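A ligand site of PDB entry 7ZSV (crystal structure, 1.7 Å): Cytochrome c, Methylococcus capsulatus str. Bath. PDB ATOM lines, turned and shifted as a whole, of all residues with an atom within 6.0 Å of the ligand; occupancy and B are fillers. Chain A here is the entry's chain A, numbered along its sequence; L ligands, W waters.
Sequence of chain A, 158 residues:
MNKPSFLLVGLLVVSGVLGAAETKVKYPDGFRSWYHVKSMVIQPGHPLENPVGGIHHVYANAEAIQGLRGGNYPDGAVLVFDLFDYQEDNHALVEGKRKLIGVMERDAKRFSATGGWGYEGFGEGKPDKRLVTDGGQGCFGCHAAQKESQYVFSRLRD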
ATOM      1  N   LYS A  38     -11.835  -8.969  17.584  1.00  0.00           N
ATOM      2  CA  LYS A  38     -12.008  -7.685  16.858  1.00  0.00           C
ATOM      3  C   LYS A  38     -10.631  -7.081  16.634  1.00  0.00           C
ATOM      4  O   LYS A  38      -9.638  -7.559  17.283  1.00  0.00           O
ATOM      5  CB  LYS A  38     -12.868  -6.666  17.622  1.00  0.00           C
ATOM      6  CG  LYS A  38     -12.255  -6.135  18.910  1.00  0.00           C
ATOM      7  CD  LYS A  38     -12.891  -4.945  19.481  1.00  0.00           C
ATOM      8  CE  LYS A  38     -12.890  -3.742  18.556  1.00  0.00           C
ATOM      9  NZ  LYS A  38     -13.477  -2.630  19.300  1.00  0.00           N
ATOM     10  N   SER A  39     -10.574  -6.096  15.752  1.00  0.00           N
ATOM     11  CA  SER A  39      -9.355  -5.306  15.489  1.00  0.00           C
ATOM     12  C   SER A  39      -9.738  -3.833  15.432  1.00  0.00           C
ATOM     13  O   SER A  39     -10.949  -3.527  15.211  1.00  0.00           O
ATOM     14  CB  SER A  39      -8.717  -5.733  14.227  1.00  0.00           C
ATOM     15  OG  SER A  39      -8.416  -7.122  14.259  1.00  0.00           O
ATOM     16  N   MET A  40      -8.722  -2.990  15.513  1.00  0.00           N
ATOM     17  CA  MET A  40      -8.834  -1.514  15.311  1.00  0.00           C
ATOM     18  C   MET A  40      -7.454  -0.998  14.894  1.00  0.00           C
ATOM     19  O   MET A  40      -6.447  -1.611  15.296  1.00  0.00           O
ATOM     20  CB  MET A  40      -9.285  -0.877  16.622  1.00  0.00           C
ATOM     21  CG  MET A  40      -9.655   0.612  16.534  1.00  0.00           C
ATOM     22  SD  MET A  40      -9.992   1.327  18.153  1.00  0.00           S
ATOM     23  CE  MET A  40     -11.550   0.585  18.597  1.00  0.00           C
ATOM     24  N   LEU A  48      -4.607   8.286  21.837  1.00  0.00           N
ATOM     25  CA  LEU A  48      -3.917   7.104  22.412  1.00  0.00           C
ATOM     26  C   LEU A  48      -2.747   6.644  21.509  1.00  0.00           C
ATOM     27  O   LEU A  48      -2.140   5.554  21.772  1.00  0.00           O
ATOM     28  CB  LEU A  48      -4.973   6.013  22.631  1.00  0.00           C
ATOM     29  CG  LEU A  48      -6.068   6.326  23.670  1.00  0.00           C
ATOM     30  CD1 LEU A  48      -6.911   5.087  23.982  1.00  0.00           C
ATOM     31  CD2 LEU A  48      -5.480   6.883  24.960  1.00  0.00           C
ATOM     32  N   HIS A  56      -4.159  -3.134  16.240  1.00  0.00           N
ATOM     33  CA  HIS A  56      -4.324  -4.118  17.341  1.00  0.00           C
ATOM     34  C   HIS A  56      -5.440  -5.125  17.036  1.00  0.00           C
ATOM     35  O   HIS A  56      -6.423  -4.805  16.346  1.00  0.00           O
ATOM     36  CB  HIS A  56      -4.448  -3.469  18.709  1.00  0.00           C
ATOM     37  CG  HIS A  56      -5.742  -2.855  18.992  1.00  0.00           C
ATOM     38  ND1 HIS A  56      -5.887  -1.492  18.959  1.00  0.00           N
ATOM     39  CD2 HIS A  56      -6.920  -3.355  19.414  1.00  0.00           C
ATOM     40  CE1 HIS A  56      -7.118  -1.176  19.337  1.00  0.00           C
ATOM     41  NE2 HIS A  56      -7.782  -2.312  19.561  1.00  0.00           N
ATOM     42  N   VAL A  58      -7.629  -8.166  19.236  1.00  0.00           N
ATOM     43  CA  VAL A  58      -8.033  -8.692  20.534  1.00  0.00           C
ATOM     44  C   VAL A  58      -8.295 -10.188  20.366  1.00  0.00           C
ATOM     45  O   VAL A  58      -9.022 -10.567  19.437  1.00  0.00           O
ATOM     46  CB  VAL A  58      -9.243  -7.949  21.083  1.00  0.00           C
ATOM     47  CG1 VAL A  58      -9.614  -8.437  22.481  1.00  0.00           C
ATOM     48  CG2 VAL A  58      -8.985  -6.463  21.097  1.00  0.00           C
ATOM     49  N   LEU A  79      -7.962 -12.242  28.093  1.00  0.00           N
ATOM     50  CA  LEU A  79      -8.071 -11.381  26.893  1.00  0.00           C
ATOM     51  C   LEU A  79      -6.660 -10.858  26.579  1.00  0.00           C
ATOM     52  O   LEU A  79      -5.915 -10.515  27.540  1.00  0.00           O
ATOM     53  CB  LEU A  79      -9.050 -10.252  27.199  1.00  0.00           C
ATOM     54  CG  LEU A  79     -10.513 -10.718  27.389  1.00  0.00           C
ATOM     55  CD1 LEU A  79     -11.293  -9.684  28.169  1.00  0.00           C
ATOM     56  CD2 LEU A  79     -11.171 -10.976  26.047  1.00  0.00           C
ATOM     57  N   VAL A  80      -6.302 -10.862  25.299  1.00  0.00           N
ATOM     58  CA  VAL A  80      -5.000 -10.329  24.827  1.00  0.00           C
ATOM     59  C   VAL A  80      -5.268  -9.203  23.826  1.00  0.00           C
ATOM     60  O   VAL A  80      -6.045  -9.382  22.876  1.00  0.00           O
ATOM     61  CB  VAL A  80      -4.102 -11.420  24.217  1.00  0.00           C
ATOM     62  CG1 VAL A  80      -2.747 -10.872  23.728  1.00  0.00           C
ATOM     63  CG2 VAL A  80      -3.915 -12.566  25.187  1.00  0.00           C
ATOM     64  N   PHE A  81      -4.585  -8.079  24.039  1.00  0.00           N
ATOM     65  CA  PHE A  81      -4.483  -6.930  23.104  1.00  0.00           C
ATOM     66  C   PHE A  81      -3.134  -7.061  22.392  1.00  0.00           C
ATOM     67  O   PHE A  81      -2.101  -6.864  23.079  1.00  0.00           O
ATOM     68  CB  PHE A  81      -4.595  -5.669  23.962  1.00  0.00           C
ATOM     69  CG  PHE A  81      -4.563  -4.349  23.230  1.00  0.00           C
ATOM     70  CD1 PHE A  81      -3.358  -3.787  22.810  1.00  0.00           C
ATOM     71  CD2 PHE A  81      -5.722  -3.616  23.025  1.00  0.00           C
ATOM     72  CE1 PHE A  81      -3.330  -2.532  22.211  1.00  0.00           C
ATOM     73  CE2 PHE A  81      -5.698  -2.359  22.402  1.00  0.00           C
ATOM     74  CZ  PHE A  81      -4.491  -1.807  22.027  1.00  0.00           C
ATOM     75  N   GLY A 102      -0.969  -6.541  25.581  1.00  0.00           N
ATOM     76  CA  GLY A 102      -1.579  -6.372  26.901  1.00  0.00           C
ATOM     77  C   GLY A 102      -2.438  -7.585  27.226  1.00  0.00           C
ATOM     78  O   GLY A 102      -2.941  -8.242  26.293  1.00  0.00           O
ATOM     79  N   VAL A 103      -2.533  -7.909  28.517  1.00  0.00           N
ATOM     80  CA  VAL A 103      -3.123  -9.169  29.014  1.00  0.00           C
ATOM     81  C   VAL A 103      -4.003  -8.840  30.214  1.00  0.00           C
ATOM     82  O   VAL A 103      -3.551  -8.157  31.171  1.00  0.00           O
ATOM     83  CB  VAL A 103      -2.080 -10.261  29.318  1.00  0.00           C
ATOM     84  CG1 VAL A 103      -2.732 -11.596  29.640  1.00  0.00           C
ATOM     85  CG2 VAL A 103      -1.132 -10.442  28.140  1.00  0.00           C
ATOM     86  N   MET A 104      -5.232  -9.375  30.145  1.00  0.00           N
ATOM     87  CA  MET A 104      -6.157  -9.339  31.290  1.00  0.00           C
ATOM     88  C   MET A 104      -6.466 -10.788  31.641  1.00  0.00           C
ATOM     89  O   MET A 104      -6.869 -11.543  30.784  1.00  0.00           O
ATOM     90  CB  MET A 104      -7.424  -8.552  30.963  1.00  0.00           C
ATOM     91  CG  MET A 104      -7.257  -7.065  30.951  1.00  0.00           C
ATOM     92  SD  MET A 104      -8.721  -6.316  30.134  1.00  0.00           S
ATOM     93  CE  MET A 104      -9.941  -6.609  31.417  1.00  0.00           C
ATOM     94  N   TYR A 119      -3.812  -7.238  35.287  1.00  0.00           N
ATOM     95  CA  TYR A 119      -3.383  -6.462  34.107  1.00  0.00           C
ATOM     96  C   TYR A 119      -1.860  -6.558  33.968  1.00  0.00           C
ATOM     97  O   TYR A 119      -1.160  -6.220  34.912  1.00  0.00           O
ATOM     98  CB  TYR A 119      -3.838  -5.010  34.241  1.00  0.00           C
ATOM     99  CG  TYR A 119      -5.335  -4.832  34.227  1.00  0.00           C
ATOM    100  CD1 TYR A 119      -6.083  -4.885  35.392  1.00  0.00           C
ATOM    101  CD2 TYR A 119      -5.984  -4.505  33.044  1.00  0.00           C
ATOM    102  CE1 TYR A 119      -7.449  -4.660  35.377  1.00  0.00           C
ATOM    103  CE2 TYR A 119      -7.343  -4.295  33.014  1.00  0.00           C
ATOM    104  CZ  TYR A 119      -8.078  -4.386  34.171  1.00  0.00           C
ATOM    105  OH  TYR A 119      -9.423  -4.207  34.112  1.00  0.00           O
ATOM    106  N   GLU A 120      -1.385  -7.000  32.798  1.00  0.00           N
ATOM    107  CA  GLU A 120       0.072  -7.064  32.519  1.00  0.00           C
ATOM    108  C   GLU A 120       0.293  -6.708  31.057  1.00  0.00           C
ATOM    109  O   GLU A 120      -0.606  -6.966  30.212  1.00  0.00           O
ATOM    110  CB  GLU A 120       0.606  -8.452  32.852  1.00  0.00           C
ATOM    111  CG  GLU A 120       2.087  -8.640  32.557  1.00  0.00           C
ATOM    112  CD  GLU A 120       2.938  -7.794  33.488  1.00  0.00           C
ATOM    113  OE1 GLU A 120       3.417  -8.335  34.506  1.00  0.00           O
ATOM    114  OE2 GLU A 120       3.079  -6.632  33.204  1.00  0.00           O
ATOM    115  N   GLY A 121       1.485  -6.190  30.778  1.00  0.00           N
ATOM    116  CA  GLY A 121       1.990  -5.944  29.433  1.00  0.00           C
ATOM    117  C   GLY A 121       3.287  -6.675  29.225  1.00  0.00           C
ATOM    118  O   GLY A 121       4.088  -6.811  30.201  1.00  0.00           O
ATOM    119  N   VAL A 132       4.271  -3.824  33.584  1.00  0.00           N
ATOM    120  CA  VAL A 132       3.397  -3.155  34.583  1.00  0.00           C
ATOM    121  C   VAL A 132       4.164  -3.073  35.894  1.00  0.00           C
ATOM    122  O   VAL A 132       4.692  -4.119  36.324  1.00  0.00           O
ATOM    123  CB  VAL A 132       2.041  -3.841  34.773  1.00  0.00           C
ATOM    124  CG1 VAL A 132       1.340  -3.406  36.059  1.00  0.00           C
ATOM    125  CG2 VAL A 132       1.138  -3.563  33.546  1.00  0.00           C
ATOM    126  N   GLY A 136      -1.111  -2.863  38.266  1.00  0.00           N
ATOM    127  CA  GLY A 136      -2.162  -2.739  37.223  1.00  0.00           C
ATOM    128  C   GLY A 136      -3.184  -1.663  37.605  1.00  0.00           C
ATOM    129  O   GLY A 136      -4.235  -1.591  36.970  1.00  0.00           O
ATOM    130  N   GLY A 138      -2.977   1.654  37.198  1.00  0.00           N
ATOM    131  CA  GLY A 138      -3.119   2.498  36.007  1.00  0.00           C
ATOM    132  C   GLY A 138      -4.046   1.868  34.958  1.00  0.00           C
ATOM    133  O   GLY A 138      -4.910   2.561  34.406  1.00  0.00           O
ATOM    134  N   CYS A 139      -3.858   0.587  34.647  1.00  0.00           N
ATOM    135  CA  CYS A 139      -4.724  -0.118  33.677  1.00  0.00           C
ATOM    136  C   CYS A 139      -6.185  -0.020  34.171  1.00  0.00           C
ATOM    137  O   CYS A 139      -7.087   0.416  33.419  1.00  0.00           O
ATOM    138  CB  CYS A 139      -4.311  -1.581  33.534  1.00  0.00           C
ATOM    139  SG  CYS A 139      -2.578  -1.726  33.145  1.00  0.00           S
ATOM    140  N   PHE A 140      -6.405  -0.523  35.379  1.00  0.00           N
ATOM    141  CA  PHE A 140      -7.715  -0.616  36.029  1.00  0.00           C
ATOM    142  C   PHE A 140      -8.394   0.780  36.038  1.00  0.00           C
ATOM    143  O   PHE A 140      -9.609   0.817  35.810  1.00  0.00           O
ATOM    144  CB  PHE A 140      -7.505  -1.226  37.404  1.00  0.00           C
ATOM    145  CG  PHE A 140      -8.779  -1.361  38.183  1.00  0.00           C
ATOM    146  CD1 PHE A 140      -9.889  -1.964  37.610  1.00  0.00           C
ATOM    147  CD2 PHE A 140      -8.876  -0.872  39.478  1.00  0.00           C
ATOM    148  CE1 PHE A 140     -11.075  -2.091  38.314  1.00  0.00           C
ATOM    149  CE2 PHE A 140     -10.065  -0.993  40.175  1.00  0.00           C
ATOM    150  CZ  PHE A 140     -11.154  -1.598  39.593  1.00  0.00           C
ATOM    151  N   CYS A 142      -8.547   3.020  33.899  1.00  0.00           N
ATOM    152  CA  CYS A 142      -9.289   3.264  32.648  1.00  0.00           C
ATOM    153  C   CYS A 142     -10.390   2.207  32.470  1.00  0.00           C
ATOM    154  O   CYS A 142     -11.535   2.580  32.191  1.00  0.00           O
ATOM    155  CB  CYS A 142      -8.319   3.306  31.500  1.00  0.00           C
ATOM    156  SG  CYS A 142      -9.075   3.892  30.057  1.00  0.00           S
ATOM    157  N   HIS A 143     -10.076   0.931  32.643  1.00  0.00           N
ATOM    158  CA  HIS A 143     -11.042  -0.174  32.491  1.00  0.00           C
ATOM    159  C   HIS A 143     -12.241  -0.021  33.456  1.00  0.00           C
ATOM    160  O   HIS A 143     -13.295  -0.623  33.159  1.00  0.00           O
ATOM    161  CB  HIS A 143     -10.306  -1.517  32.562  1.00  0.00           C
ATOM    162  CG  HIS A 143      -9.567  -1.801  31.295  1.00  0.00           C
ATOM    163  ND1 HIS A 143     -10.010  -2.732  30.384  1.00  0.00           N
ATOM    164  CD2 HIS A 143      -8.476  -1.220  30.739  1.00  0.00           C
ATOM    165  CE1 HIS A 143      -9.182  -2.742  29.329  1.00  0.00           C
ATOM    166  NE2 HIS A 143      -8.218  -1.833  29.507  1.00  0.00           N
ATOM    167  N   TYR A 151     -15.478  -4.745  32.969  1.00  0.00           N
ATOM    168  CA  TYR A 151     -14.186  -4.031  32.767  1.00  0.00           C
ATOM    169  C   TYR A 151     -13.582  -4.309  31.400  1.00  0.00           C
ATOM    170  O   TYR A 151     -12.419  -3.889  31.196  1.00  0.00           O
ATOM    171  CB  TYR A 151     -13.201  -4.410  33.873  1.00  0.00           C
ATOM    172  CG  TYR A 151     -13.728  -4.100  35.257  1.00  0.00           C
ATOM    173  CD1 TYR A 151     -13.834  -2.794  35.684  1.00  0.00           C
ATOM    174  CD2 TYR A 151     -14.165  -5.112  36.099  1.00  0.00           C
ATOM    175  CE1 TYR A 151     -14.329  -2.487  36.949  1.00  0.00           C
ATOM    176  CE2 TYR A 151     -14.649  -4.832  37.364  1.00  0.00           C
ATOM    177  CZ  TYR A 151     -14.723  -3.510  37.783  1.00  0.00           C
ATOM    178  OH  TYR A 151     -15.189  -3.190  39.022  1.00  0.00           O
ATOM    179  N   VAL A 152     -14.356  -4.899  30.471  1.00  0.00           N
ATOM    180  CA  VAL A 152     -13.965  -5.244  29.073  1.00  0.00           C
ATOM    181  C   VAL A 152     -14.587  -4.241  28.104  1.00  0.00           C
ATOM    182  O   VAL A 152     -15.804  -4.010  28.196  1.00  0.00           O
ATOM    183  CB  VAL A 152     -14.368  -6.690  28.764  1.00  0.00           C
ATOM    184  CG1 VAL A 152     -14.041  -7.077  27.338  1.00  0.00           C
ATOM    185  CG2 VAL A 152     -13.713  -7.638  29.767  1.00  0.00           C
ATOM    186  N   PHE A 153     -13.773  -3.582  27.272  1.00  0.00           N
ATOM    187  CA  PHE A 153     -14.231  -2.638  26.232  1.00  0.00           C
ATOM    188  C   PHE A 153     -14.757  -3.409  25.026  1.00  0.00           C
ATOM    189  O   PHE A 153     -15.789  -3.043  24.468  1.00  0.00           O
ATOM    190  CB  PHE A 153     -13.090  -1.712  25.771  1.00  0.00           C
ATOM    191  CG  PHE A 153     -12.706  -0.649  26.755  1.00  0.00           C
ATOM    192  CD1 PHE A 153     -11.680  -0.854  27.673  1.00  0.00           C
ATOM    193  CD2 PHE A 153     -13.435   0.535  26.831  1.00  0.00           C
ATOM    194  CE1 PHE A 153     -11.343   0.130  28.606  1.00  0.00           C
ATOM    195  CE2 PHE A 153     -13.112   1.517  27.767  1.00  0.00           C
ATOM    196  CZ  PHE A 153     -12.035   1.337  28.623  1.00  0.00           C
ATOM    197  N   SER A 154     -14.008  -4.419  24.595  1.00  0.00           N
ATOM    198  CA  SER A 154     -14.187  -5.129  23.308  1.00  0.00           C
ATOM    199  C   SER A 154     -15.581  -5.775  23.316  1.00  0.00           C
ATOM    200  O   SER A 154     -15.979  -6.315  24.388  1.00  0.00           O
ATOM    201  CB  SER A 154     -13.115  -6.154  23.087  1.00  0.00           C
ATOM    202  OG  SER A 154     -11.879  -5.538  22.769  1.00  0.00           O
ATOM    203  N   ARG A 155     -16.309  -5.658  22.197  1.00  0.00           N
ATOM    204  CA  ARG A 155     -17.598  -6.371  21.999  1.00  0.00           C
ATOM    205  C   ARG A 155     -17.398  -7.429  20.951  1.00  0.00           C
ATOM    206  O   ARG A 155     -16.738  -7.180  19.880  1.00  0.00           O
ATOM    207  CB  ARG A 155     -18.742  -5.421  21.610  1.00  0.00           C
ATOM    208  CG  ARG A 155     -18.861  -4.219  22.540  1.00  0.00           C
ATOM    209  CD  ARG A 155     -19.571  -4.559  23.831  1.00  0.00           C
ATOM    210  NE  ARG A 155     -19.572  -3.348  24.652  1.00  0.00           N
ATOM    211  CZ  ARG A 155     -18.910  -3.161  25.790  1.00  0.00           C
ATOM    212  NH1 ARG A 155     -18.185  -4.125  26.347  1.00  0.00           N
ATOM    213  NH2 ARG A 155     -18.969  -1.985  26.375  1.00  0.00           N
HETATM  214 FE1  LIG L   1      -6.845  -1.511  28.003  1.00  0.00          FE
HETATM  215  C1  LIG L   1      -8.626  -3.056  25.529  1.00  0.00           C
HETATM  216  C2  LIG L   1      -5.181  -4.452  28.646  1.00  0.00           C
HETATM  217  C3  LIG L   1      -4.628   0.162  29.839  1.00  0.00           C
HETATM  218  C4  LIG L   1      -8.386   1.354  27.286  1.00  0.00           C
HETATM  219  N1  LIG L   1      -6.854  -3.427  27.202  1.00  0.00           N
HETATM  220  C5  LIG L   1      -7.744  -3.891  26.264  1.00  0.00           C
HETATM  221  C6  LIG L   1      -7.722  -5.308  26.170  1.00  0.00           C
HETATM  222  C7  LIG L   1      -6.718  -5.724  27.067  1.00  0.00           C
HETATM  223  C8  LIG L   1      -6.221  -4.543  27.675  1.00  0.00           C
HETATM  224  C9  LIG L   1      -6.286  -7.135  27.293  1.00  0.00           C
HETATM  225  C10 LIG L   1      -8.653  -6.167  25.399  1.00  0.00           C
HETATM  226  C11 LIG L   1      -9.899  -6.459  26.279  1.00  0.00           C
HETATM  227  C12 LIG L   1     -10.901  -5.292  26.317  1.00  0.00           C
HETATM  228  O1  LIG L   1     -11.395  -4.891  25.214  1.00  0.00           O
HETATM  229  O2  LIG L   1     -11.146  -4.730  27.411  1.00  0.00           O
HETATM  230  N2  LIG L   1      -5.183  -2.061  29.137  1.00  0.00           N
HETATM  231  C13 LIG L   1      -4.694  -3.299  29.300  1.00  0.00           C
HETATM  232  C14 LIG L   1      -3.561  -3.246  30.185  1.00  0.00           C
HETATM  233  C15 LIG L   1      -3.375  -1.924  30.552  1.00  0.00           C
HETATM  234  C16 LIG L   1      -4.424  -1.249  29.841  1.00  0.00           C
HETATM  235  C17 LIG L   1      -2.727  -4.436  30.538  1.00  0.00           C
HETATM  236  C18 LIG L   1      -2.317  -1.280  31.453  1.00  0.00           C
HETATM  237  C19 LIG L   1      -0.875  -1.664  31.049  1.00  0.00           C
HETATM  238  N3  LIG L   1      -6.534   0.458  28.410  1.00  0.00           N
HETATM  239  C20 LIG L   1      -5.645   0.951  29.291  1.00  0.00           C
HETATM  240  C21 LIG L   1      -5.879   2.321  29.584  1.00  0.00           C
HETATM  241  C22 LIG L   1      -7.015   2.698  28.854  1.00  0.00           C
HETATM  242  C23 LIG L   1      -7.329   1.509  28.158  1.00  0.00           C
HETATM  243  C24 LIG L   1      -5.004   3.151  30.467  1.00  0.00           C
HETATM  244  C25 LIG L   1      -7.829   3.983  28.786  1.00  0.00           C
HETATM  245  C26 LIG L   1      -7.013   5.253  29.013  1.00  0.00           C
HETATM  246  N4  LIG L   1      -8.130  -0.934  26.552  1.00  0.00           N
HETATM  247  C27 LIG L   1      -8.654   0.305  26.399  1.00  0.00           C
HETATM  248  C28 LIG L   1      -9.547   0.386  25.299  1.00  0.00           C
HETATM  249  C29 LIG L   1      -9.640  -0.910  24.780  1.00  0.00           C
HETATM  250  C30 LIG L   1      -8.755  -1.671  25.603  1.00  0.00           C
HETATM  251  C31 LIG L   1     -10.304   1.595  24.779  1.00  0.00           C
HETATM  252  C32 LIG L   1     -10.519  -1.369  23.658  1.00  0.00           C
HETATM  253  C33 LIG L   1      -9.767  -1.516  22.301  1.00  0.00           C
HETATM  254  C34 LIG L   1     -10.669  -1.894  21.159  1.00  0.00           C
HETATM  255  O3  LIG L   1     -10.225  -2.343  20.098  1.00  0.00           O
HETATM  256  O4  LIG L   1     -11.933  -1.790  21.293  1.00  0.00           O
HETATM  257  O   HOH W   1      -7.216   1.613  23.266  1.00  0.00           O
HETATM  258  O   HOH W   2      -4.479  -1.342  26.020  1.00  0.00           O
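Residues that only touch the ligand: Met 40, Val 58, Leu 79, Phe 81, Gly 102, Val 103, Met 104, Tyr 119, Glu 120, Val 132, Gly 138 and Val 152.
Hydrophobic or aromatic side chains within 4 Å of the ligand: Met 40, His 56, Val 58, Leu 79, Phe 81, Met 104, Tyr 119, Val 132, His 143, Val 152 and Phe 153.
19 residues have an atom within 4 Å of the ligand: Lys 38, Met 40, His 56, Val 58, Leu 79, Phe 81, Gly 102, Val 103, Met 104, Tyr 119, Glu 120, Val 132, Gly 138, Cys 139, Cys 142, His 143, Val 152, Phe 153 and Ser 154.
O of Tyr 151 lies within hydrogen-bond range of ND1 of His 143 (2.8 Å).
O of Met 40 is in hydrogen-bond range of N of His 56, 2.9 Å away.
N of Val 58 is in hydrogen-bond range of O of Lys 38 (2.9 Å).
The backbone carbonyl oxygen of Phe 153 is in hydrogen-bond range of the guanidinium group of Arg 155, 3.2 Å away.
N of Val 132 sits at hydrogen-bond distance from OE2 of Glu 120, at 3.1 Å.
O of Glu 120 lies within hydrogen-bond range of N of Val 103 (2.7 Å).
The backbone carbonyl oxygen (O) of Leu 79 lies within hydrogen-bond range of the backbone NH (N) of Met 104.
N of Gly 102 lies within hydrogen-bond range of O of Phe 81 (2.8 Å).
A carbon (C18) of the ligand is bonded to the side-chain sulfur (SG) of Cys 139, at 1.8 Å.
C25 of the ligand is bonded to SG of Cys 142 (1.8 Å).
An iron atom (FE1) of the ligand is bound by a ring nitrogen (NE2) of His 143 (2.1 Å).
O3 of the ligand is in hydrogen-bond range of NE2 of His 56 (2.5 Å).
An oxygen (O1) of the ligand is in hydrogen-bond range of the backbone NH of Ser 154.
The side-chain hydroxyl of Ser 154 is in hydrogen-bond range of an oxygen (O1) of the ligand, 2.6 Å away.
NZ of Lys 38 lies within salt-bridge range of O4 of the ligand (2.7 Å).
An oxygen (O2) of the ligand lies within hydrogen-bond range of the backbone NH (N) of Phe 153, at 2.9 Å.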
